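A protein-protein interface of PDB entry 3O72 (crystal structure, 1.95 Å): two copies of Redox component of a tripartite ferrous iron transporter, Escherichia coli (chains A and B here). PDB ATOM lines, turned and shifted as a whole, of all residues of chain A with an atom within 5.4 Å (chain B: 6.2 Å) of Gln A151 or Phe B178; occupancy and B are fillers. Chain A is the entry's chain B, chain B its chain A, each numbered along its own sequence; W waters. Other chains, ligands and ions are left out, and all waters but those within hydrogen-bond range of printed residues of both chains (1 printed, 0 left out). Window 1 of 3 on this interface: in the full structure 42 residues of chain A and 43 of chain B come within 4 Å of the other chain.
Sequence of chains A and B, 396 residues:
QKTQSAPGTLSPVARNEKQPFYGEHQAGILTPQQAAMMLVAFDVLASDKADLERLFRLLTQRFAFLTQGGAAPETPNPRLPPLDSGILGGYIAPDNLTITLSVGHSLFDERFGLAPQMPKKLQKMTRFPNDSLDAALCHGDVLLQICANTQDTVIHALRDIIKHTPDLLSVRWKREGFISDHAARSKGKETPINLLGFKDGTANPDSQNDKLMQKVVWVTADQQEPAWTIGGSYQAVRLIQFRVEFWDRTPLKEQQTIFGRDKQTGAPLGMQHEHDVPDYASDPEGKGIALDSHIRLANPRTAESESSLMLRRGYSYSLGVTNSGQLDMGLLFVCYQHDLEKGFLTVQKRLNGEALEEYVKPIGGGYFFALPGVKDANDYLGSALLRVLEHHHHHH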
ATOM      1  N   ALA A  36     -24.017   4.082   8.234  1.00  0.00           N
ATOM      2  CA  ALA A  36     -23.863   5.417   8.789  1.00  0.00           C
ATOM      3  C   ALA A  36     -23.411   5.314  10.222  1.00  0.00           C
ATOM      4  O   ALA A  36     -23.792   4.400  10.940  1.00  0.00           O
ATOM      5  CB  ALA A  36     -25.175   6.209   8.707  1.00  0.00           C
ATOM      6  N   ASN A 149     -28.426   2.100   9.723  1.00  0.00           N
ATOM      7  CA  ASN A 149     -28.487   2.073   8.266  1.00  0.00           C
ATOM      8  C   ASN A 149     -28.419   3.470   7.664  1.00  0.00           C
ATOM      9  O   ASN A 149     -27.868   3.651   6.579  1.00  0.00           O
ATOM     10  CB  ASN A 149     -29.744   1.349   7.757  1.00  0.00           C
ATOM     11  CG  ASN A 149     -29.741  -0.119   8.090  1.00  0.00           C
ATOM     12  OD1 ASN A 149     -28.699  -0.777   8.062  1.00  0.00           O
ATOM     13  ND2 ASN A 149     -30.909  -0.647   8.414  1.00  0.00           N
ATOM     14  N   THR A 150     -28.960   4.462   8.377  1.00  0.00           N
ATOM     15  CA  THR A 150     -29.061   5.812   7.835  1.00  0.00           C
ATOM     16  C   THR A 150     -28.679   6.906   8.829  1.00  0.00           C
ATOM     17  O   THR A 150     -28.848   6.762  10.037  1.00  0.00           O
ATOM     18  CB  THR A 150     -30.502   6.119   7.322  1.00  0.00           C
ATOM     19  OG1 THR A 150     -31.419   6.109   8.427  1.00  0.00           O
ATOM     20  CG2 THR A 150     -30.943   5.081   6.305  1.00  0.00           C
ATOM     21  N   GLN A 151     -28.187   8.012   8.291  1.00  0.00           N
ATOM     22  CA  GLN A 151     -27.764   9.165   9.072  1.00  0.00           C
ATOM     23  C   GLN A 151     -28.899   9.770   9.915  1.00  0.00           C
ATOM     24  O   GLN A 151     -28.667  10.272  11.011  1.00  0.00           O
ATOM     25  CB  GLN A 151     -27.175  10.207   8.122  1.00  0.00           C
ATOM     26  CG  GLN A 151     -26.771  11.513   8.744  1.00  0.00           C
ATOM     27  CD  GLN A 151     -25.824  12.307   7.841  1.00  0.00           C
ATOM     28  OE1 GLN A 151     -25.811  12.128   6.617  1.00  0.00           O
ATOM     29  NE2 GLN A 151     -25.030  13.190   8.446  1.00  0.00           N
ATOM     30  N   ASP A 152     -30.133   9.706   9.421  1.00  0.00           N
ATOM     31  CA  ASP A 152     -31.245  10.325  10.145  1.00  0.00           C
ATOM     32  C   ASP A 152     -31.436   9.611  11.477  1.00  0.00           C
ATOM     33  O   ASP A 152     -31.683  10.246  12.512  1.00  0.00           O
ATOM     34  CB  ASP A 152     -32.531  10.252   9.328  1.00  0.00           C
ATOM     35  CG  ASP A 152     -32.259  10.090   7.851  1.00  0.00           C
ATOM     36  OD1 ASP A 152     -31.878  11.092   7.206  1.00  0.00           O
ATOM     37  OD2 ASP A 152     -32.399   8.954   7.344  1.00  0.00           O
ATOM     38  N   THR A 153     -31.300   8.290  11.443  1.00  0.00           N
ATOM     39  CA  THR A 153     -31.466   7.494  12.650  1.00  0.00           C
ATOM     40  C   THR A 153     -30.410   7.855  13.685  1.00  0.00           C
ATOM     41  O   THR A 153     -30.705   7.991  14.871  1.00  0.00           O
ATOM     42  CB  THR A 153     -31.423   5.982  12.336  1.00  0.00           C
ATOM     43  OG1 THR A 153     -32.493   5.666  11.443  1.00  0.00           O
ATOM     44  CG2 THR A 153     -31.578   5.157  13.606  1.00  0.00           C
ATOM     45  N   VAL A 154     -29.181   8.033  13.221  1.00  0.00           N
ATOM     46  CA  VAL A 154     -28.064   8.341  14.100  1.00  0.00           C
ATOM     47  C   VAL A 154     -28.238   9.725  14.758  1.00  0.00           C
ATOM     48  O   VAL A 154     -28.115   9.868  15.972  1.00  0.00           O
ATOM     49  CB  VAL A 154     -26.738   8.227  13.305  1.00  0.00           C
ATOM     50  CG1 VAL A 154     -25.559   8.681  14.117  1.00  0.00           C
ATOM     51  CG2 VAL A 154     -26.543   6.765  12.821  1.00  0.00           C
ATOM     52  N   ILE A 155     -28.548  10.738  13.960  1.00  0.00           N
ATOM     53  CA  ILE A 155     -28.777  12.101  14.475  1.00  0.00           C
ATOM     54  C   ILE A 155     -29.959  12.149  15.432  1.00  0.00           C
ATOM     55  O   ILE A 155     -29.925  12.827  16.454  1.00  0.00           O
ATOM     56  CB  ILE A 155     -29.056  13.081  13.323  1.00  0.00           C
ATOM     57  CG1 ILE A 155     -27.793  13.263  12.476  1.00  0.00           C
ATOM     58  CG2 ILE A 155     -29.567  14.440  13.868  1.00  0.00           C
ATOM     59  CD1 ILE A 155     -28.041  13.871  11.125  1.00  0.00           C
ATOM     60  N   HIS A 156     -31.015  11.424  15.093  1.00  0.00           N
ATOM     61  CA  HIS A 156     -32.177  11.339  15.963  1.00  0.00           C
ATOM     62  C   HIS A 156     -31.798  10.772  17.316  1.00  0.00           C
ATOM     63  O   HIS A 156     -32.223  11.287  18.356  1.00  0.00           O
ATOM     64  CB  HIS A 156     -33.304  10.486  15.357  1.00  0.00           C
ATOM     65  CG  HIS A 156     -34.431  10.256  16.318  1.00  0.00           C
ATOM     66  ND1 HIS A 156     -34.459   9.187  17.188  1.00  0.00           N
ATOM     67  CD2 HIS A 156     -35.525  11.002  16.600  1.00  0.00           C
ATOM     68  CE1 HIS A 156     -35.537   9.270  17.953  1.00  0.00           C
ATOM     69  NE2 HIS A 156     -36.200  10.362  17.616  1.00  0.00           N
ATOM     70  N   GLU A 176     -19.181  12.405  12.064  1.00  0.00           N
ATOM     71  CA  GLU A 176     -20.014  11.402  11.427  1.00  0.00           C
ATOM     72  C   GLU A 176     -19.261  10.766  10.268  1.00  0.00           C
ATOM     73  O   GLU A 176     -18.425  11.406   9.645  1.00  0.00           O
ATOM     74  CB  GLU A 176     -21.328  12.025  10.962  1.00  0.00           C
ATOM     75  CG  GLU A 176     -22.139  12.649  12.109  1.00  0.00           C
ATOM     76  CD  GLU A 176     -23.545  13.054  11.703  1.00  0.00           C
ATOM     77  OE1 GLU A 176     -24.250  12.244  11.063  1.00  0.00           O
ATOM     78  OE2 GLU A 176     -23.962  14.175  12.050  1.00  0.00           O
ATOM     79  N   GLN B  34     -32.491  13.440  -4.953  1.00  0.00           N
ATOM     80  CA  GLN B  34     -31.799  12.231  -4.524  1.00  0.00           C
ATOM     81  C   GLN B  34     -31.336  12.383  -3.061  1.00  0.00           C
ATOM     82  O   GLN B  34     -31.371  13.482  -2.497  1.00  0.00           O
ATOM     83  CB  GLN B  34     -30.616  11.955  -5.455  1.00  0.00           C
ATOM     84  CG  GLN B  34     -30.937  12.085  -6.943  1.00  0.00           C
ATOM     85  CD  GLN B  34     -30.571  13.442  -7.506  1.00  0.00           C
ATOM     86  OE1 GLN B  34     -30.911  14.484  -6.931  1.00  0.00           O
ATOM     87  NE2 GLN B  34     -29.882  13.443  -8.650  1.00  0.00           N
ATOM     88  N   ALA B  35     -30.908  11.291  -2.441  1.00  0.00           N
ATOM     89  CA  ALA B  35     -30.672  11.308  -0.997  1.00  0.00           C
ATOM     90  C   ALA B  35     -29.405  12.052  -0.568  1.00  0.00           C
ATOM     91  O   ALA B  35     -29.309  12.527   0.570  1.00  0.00           O
ATOM     92  CB  ALA B  35     -30.664   9.895  -0.437  1.00  0.00           C
ATOM     93  N   ALA B  36     -28.422  12.120  -1.459  1.00  0.00           N
ATOM     94  CA  ALA B  36     -27.144  12.702  -1.102  1.00  0.00           C
ATOM     95  C   ALA B  36     -26.830  13.852  -2.033  1.00  0.00           C
ATOM     96  O   ALA B  36     -27.193  13.831  -3.208  1.00  0.00           O
ATOM     97  CB  ALA B  36     -26.045  11.660  -1.153  1.00  0.00           C
ATOM     98  N   MET B  37     -26.152  14.865  -1.515  1.00  0.00           N
ATOM     99  CA  MET B  37     -25.723  15.944  -2.386  1.00  0.00           C
ATOM    100  C   MET B  37     -24.502  16.683  -1.869  1.00  0.00           C
ATOM    101  O   MET B  37     -24.106  16.546  -0.710  1.00  0.00           O
ATOM    102  CB  MET B  37     -26.864  16.921  -2.634  1.00  0.00           C
ATOM    103  CG  MET B  37     -27.268  17.732  -1.433  1.00  0.00           C
ATOM    104  SD  MET B  37     -26.379  19.479  -1.404  1.00  0.00           S
ATOM    105  CE  MET B  37     -27.335  20.328  -2.913  1.00  0.00           C
ATOM    106  N   GLN B 151     -23.546   9.033  -1.058  1.00  0.00           N
ATOM    107  CA  GLN B 151     -22.436   9.951  -0.885  1.00  0.00           C
ATOM    108  C   GLN B 151     -21.194   9.488  -1.648  1.00  0.00           C
ATOM    109  O   GLN B 151     -20.426  10.305  -2.141  1.00  0.00           O
ATOM    110  CB  GLN B 151     -22.109  10.068   0.606  1.00  0.00           C
ATOM    111  CG  GLN B 151     -21.080  11.121   0.956  1.00  0.00           C
ATOM    112  CD  GLN B 151     -21.053  11.428   2.458  1.00  0.00           C
ATOM    113  OE1 GLN B 151     -21.643  10.695   3.260  1.00  0.00           O
ATOM    114  NE2 GLN B 151     -20.366  12.515   2.838  1.00  0.00           N
ATOM    115  N   GLU B 176     -21.602  19.147   2.122  1.00  0.00           N
ATOM    116  CA  GLU B 176     -22.444  18.019   1.757  1.00  0.00           C
ATOM    117  C   GLU B 176     -23.735  18.007   2.586  1.00  0.00           C
ATOM    118  O   GLU B 176     -23.759  18.463   3.746  1.00  0.00           O
ATOM    119  CB  GLU B 176     -21.680  16.679   1.897  1.00  0.00           C
ATOM    120  CG  GLU B 176     -20.450  16.643   0.997  1.00  0.00           C
ATOM    121  CD  GLU B 176     -19.717  15.312   0.981  1.00  0.00           C
ATOM    122  OE1 GLU B 176     -20.362  14.248   0.829  1.00  0.00           O
ATOM    123  OE2 GLU B 176     -18.478  15.344   1.070  1.00  0.00           O
ATOM    124  N   GLY B 177     -24.800  17.500   1.977  1.00  0.00           N
ATOM    125  CA  GLY B 177     -26.084  17.402   2.645  1.00  0.00           C
ATOM    126  C   GLY B 177     -26.860  16.147   2.278  1.00  0.00           C
ATOM    127  O   GLY B 177     -26.412  15.336   1.453  1.00  0.00           O
ATOM    128  N   PHE B 178     -28.030  15.988   2.882  1.00  0.00           N
ATOM    129  CA  PHE B 178     -28.835  14.779   2.693  1.00  0.00           C
ATOM    130  C   PHE B 178     -30.314  15.059   2.917  1.00  0.00           C
ATOM    131  O   PHE B 178     -30.672  16.046   3.555  1.00  0.00           O
ATOM    132  CB  PHE B 178     -28.409  13.714   3.702  1.00  0.00           C
ATOM    133  CG  PHE B 178     -28.642  14.126   5.143  1.00  0.00           C
ATOM    134  CD1 PHE B 178     -29.797  13.746   5.808  1.00  0.00           C
ATOM    135  CD2 PHE B 178     -27.715  14.904   5.815  1.00  0.00           C
ATOM    136  CE1 PHE B 178     -30.026  14.138   7.138  1.00  0.00           C
ATOM    137  CE2 PHE B 178     -27.936  15.302   7.146  1.00  0.00           C
ATOM    138  CZ  PHE B 178     -29.090  14.904   7.802  1.00  0.00           C
ATOM    139  N   ILE B 179     -31.164  14.176   2.397  1.00  0.00           N
ATOM    140  CA  ILE B 179     -32.527  14.014   2.902  1.00  0.00           C
ATOM    141  C   ILE B 179     -32.692  12.532   3.258  1.00  0.00           C
ATOM    142  O   ILE B 179     -31.844  11.728   2.906  1.00  0.00           O
ATOM    143  CB  ILE B 179     -33.609  14.457   1.870  1.00  0.00           C
ATOM    144  CG1 ILE B 179     -33.518  13.649   0.573  1.00  0.00           C
ATOM    145  CG2 ILE B 179     -33.544  15.965   1.604  1.00  0.00           C
ATOM    146  CD1 ILE B 179     -34.739  13.843  -0.343  1.00  0.00           C
ATOM    147  N   SER B 180     -33.771  12.150   3.938  1.00  0.00           N
ATOM    148  CA  SER B 180     -33.950  10.732   4.294  1.00  0.00           C
ATOM    149  C   SER B 180     -34.075   9.858   3.051  1.00  0.00           C
ATOM    150  O   SER B 180     -34.621  10.288   2.028  1.00  0.00           O
ATOM    151  CB  SER B 180     -35.180  10.519   5.170  1.00  0.00           C
ATOM    152  OG  SER B 180     -36.360  10.559   4.382  1.00  0.00           O
ATOM    153  N   LEU B 195     -34.115  19.282   9.822  1.00  0.00           N
ATOM    154  CA  LEU B 195     -33.559  18.942  11.133  1.00  0.00           C
ATOM    155  C   LEU B 195     -34.182  19.720  12.302  1.00  0.00           C
ATOM    156  O   LEU B 195     -33.789  19.520  13.445  1.00  0.00           O
ATOM    157  CB  LEU B 195     -32.024  19.100  11.129  1.00  0.00           C
ATOM    158  CG  LEU B 195     -31.330  18.025  10.280  1.00  0.00           C
ATOM    159  CD1 LEU B 195     -29.828  18.278  10.139  1.00  0.00           C
ATOM    160  CD2 LEU B 195     -31.597  16.612  10.873  1.00  0.00           C
ATOM    161  N   GLY B 314     -33.819  22.118  -1.253  1.00  0.00           N
ATOM    162  CA  GLY B 314     -32.864  22.194  -0.160  1.00  0.00           C
ATOM    163  C   GLY B 314     -32.555  20.852   0.485  1.00  0.00           C
ATOM    164  O   GLY B 314     -33.360  19.918   0.402  1.00  0.00           O
ATOM    165  N   TYR B 315     -31.400  20.773   1.151  1.00  0.00           N
ATOM    166  CA  TYR B 315     -30.951  19.558   1.835  1.00  0.00           C
ATOM    167  C   TYR B 315     -30.513  19.853   3.267  1.00  0.00           C
ATOM    168  O   TYR B 315     -30.050  20.940   3.564  1.00  0.00           O
ATOM    169  CB  TYR B 315     -29.756  18.949   1.100  1.00  0.00           C
ATOM    170  CG  TYR B 315     -30.114  18.179  -0.149  1.00  0.00           C
ATOM    171  CD1 TYR B 315     -30.067  16.788  -0.165  1.00  0.00           C
ATOM    172  CD2 TYR B 315     -30.485  18.836  -1.311  1.00  0.00           C
ATOM    173  CE1 TYR B 315     -30.401  16.081  -1.279  1.00  0.00           C
ATOM    174  CE2 TYR B 315     -30.813  18.128  -2.455  1.00  0.00           C
ATOM    175  CZ  TYR B 315     -30.772  16.745  -2.430  1.00  0.00           C
ATOM    176  OH  TYR B 315     -31.090  16.016  -3.564  1.00  0.00           O
ATOM    177  N   SER B 316     -30.615  18.864   4.141  1.00  0.00           N
ATOM    178  CA  SER B 316     -30.142  19.018   5.513  1.00  0.00           C
ATOM    179  C   SER B 316     -28.634  18.866   5.530  1.00  0.00           C
ATOM    180  O   SER B 316     -28.082  18.210   4.664  1.00  0.00           O
ATOM    181  CB  SER B 316     -30.761  17.943   6.389  1.00  0.00           C
ATOM    182  OG  SER B 316     -32.143  18.178   6.609  1.00  0.00           O
ATOM    183  N   TYR B 317     -27.958  19.478   6.498  1.00  0.00           N
ATOM    184  CA  TYR B 317     -26.545  19.143   6.733  1.00  0.00           C
ATOM    185  C   TYR B 317     -26.234  18.943   8.206  1.00  0.00           C
ATOM    186  O   TYR B 317     -26.895  19.488   9.082  1.00  0.00           O
ATOM    187  CB  TYR B 317     -25.583  20.165   6.097  1.00  0.00           C
ATOM    188  CG  TYR B 317     -25.385  21.435   6.890  1.00  0.00           C
ATOM    189  CD1 TYR B 317     -24.460  21.493   7.936  1.00  0.00           C
ATOM    190  CD2 TYR B 317     -26.109  22.580   6.593  1.00  0.00           C
ATOM    191  CE1 TYR B 317     -24.272  22.662   8.672  1.00  0.00           C
ATOM    192  CE2 TYR B 317     -25.919  23.762   7.317  1.00  0.00           C
ATOM    193  CZ  TYR B 317     -25.001  23.784   8.354  1.00  0.00           C
ATOM    194  OH  TYR B 317     -24.807  24.944   9.059  1.00  0.00           O
ATOM    195  N   SER B 318     -25.220  18.131   8.471  1.00  0.00           N
ATOM    196  CA  SER B 318     -24.778  17.887   9.838  1.00  0.00           C
ATOM    197  C   SER B 318     -23.257  17.733   9.823  1.00  0.00           C
ATOM    198  O   SER B 318     -22.727  16.912   9.077  1.00  0.00           O
ATOM    199  CB  SER B 318     -25.468  16.632  10.377  1.00  0.00           C
ATOM    200  OG  SER B 318     -25.057  16.348  11.703  1.00  0.00           O
ATOM    201  N   LEU B 332     -28.814  23.350   3.709  1.00  0.00           N
ATOM    202  CA  LEU B 332     -28.275  23.849   2.461  1.00  0.00           C
ATOM    203  C   LEU B 332     -29.492  24.249   1.617  1.00  0.00           C
ATOM    204  O   LEU B 332     -30.129  23.413   0.979  1.00  0.00           O
ATOM    205  CB  LEU B 332     -27.414  22.788   1.754  1.00  0.00           C
ATOM    206  CG  LEU B 332     -26.334  22.092   2.593  1.00  0.00           C
ATOM    207  CD1 LEU B 332     -25.567  21.065   1.750  1.00  0.00           C
ATOM    208  CD2 LEU B 332     -25.369  23.103   3.184  1.00  0.00           C
HETATM  209  O   HOH W   1     -22.509  14.424   7.483  1.00  0.00           O
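The side-chain hydroxyl of Ser B318 lies within hydrogen-bond range of the side-chain carboxylate of Glu A176 (2.5 Å).
The side-chain carboxylate (OE1) of Glu A176 sits at hydrogen-bond distance from the side-chain amide nitrogen (NE2) of Gln A151, 2.9 Å away.
The side-chain hydroxyl (OG1) of Thr A150 lies within hydrogen-bond range of the side-chain carboxylate (OD2) of Asp A152 (3.2 Å).
N of Phe B178 is in hydrogen-bond range of O of Ser B316 (2.8 Å).
Among the printed residues, merely in contact across the chains: Gln A151 with Phe B178, Gln A151 with Ser B318, Asp A152 with Phe B178, Asp A152 with Ser B180, Ile A155 with Phe B178 and Ile A155 with Ser B318.
Of the printed residues of chain B, Asp A152 touches Phe B178 (3.6 Å) and Ser B180 (3.6 Å).
Of chain A, only Gln A151, Asp A152 and Ile A155 come within 4 Å of Phe B178.
Printed residues of chain A within 4 Å of Ser B180: Asp A152 (3.6 Å).
Printed residues of chain A within 4 Å of Ser B318: Gln A151 (3.97 Å), Ile A155 (3.8 Å) and Glu A176 (2.5 Å).
The nearest printed residue of chain A that does not touch Ser B180 is Thr A150 (6.5 Å).
Hydrophobic or aromatic side chains of chain B that line the printed part of chain A: Phe B178.
Among the printed residues, no Asp or Glu carboxylate lies within 4 Å of a Lys or Arg side-chain nitrogen of the other chain.
3 positions are printed for both chains.
Of the 7 pairs that touch across the chains among the printed residues, none has its exchanged pair printed and touching as well.
Water W1 bridges the backbone carbonyl oxygen of Ser B318 (3.0 Å) and the side-chain amide nitrogen of Gln A151 (3.0 Å).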
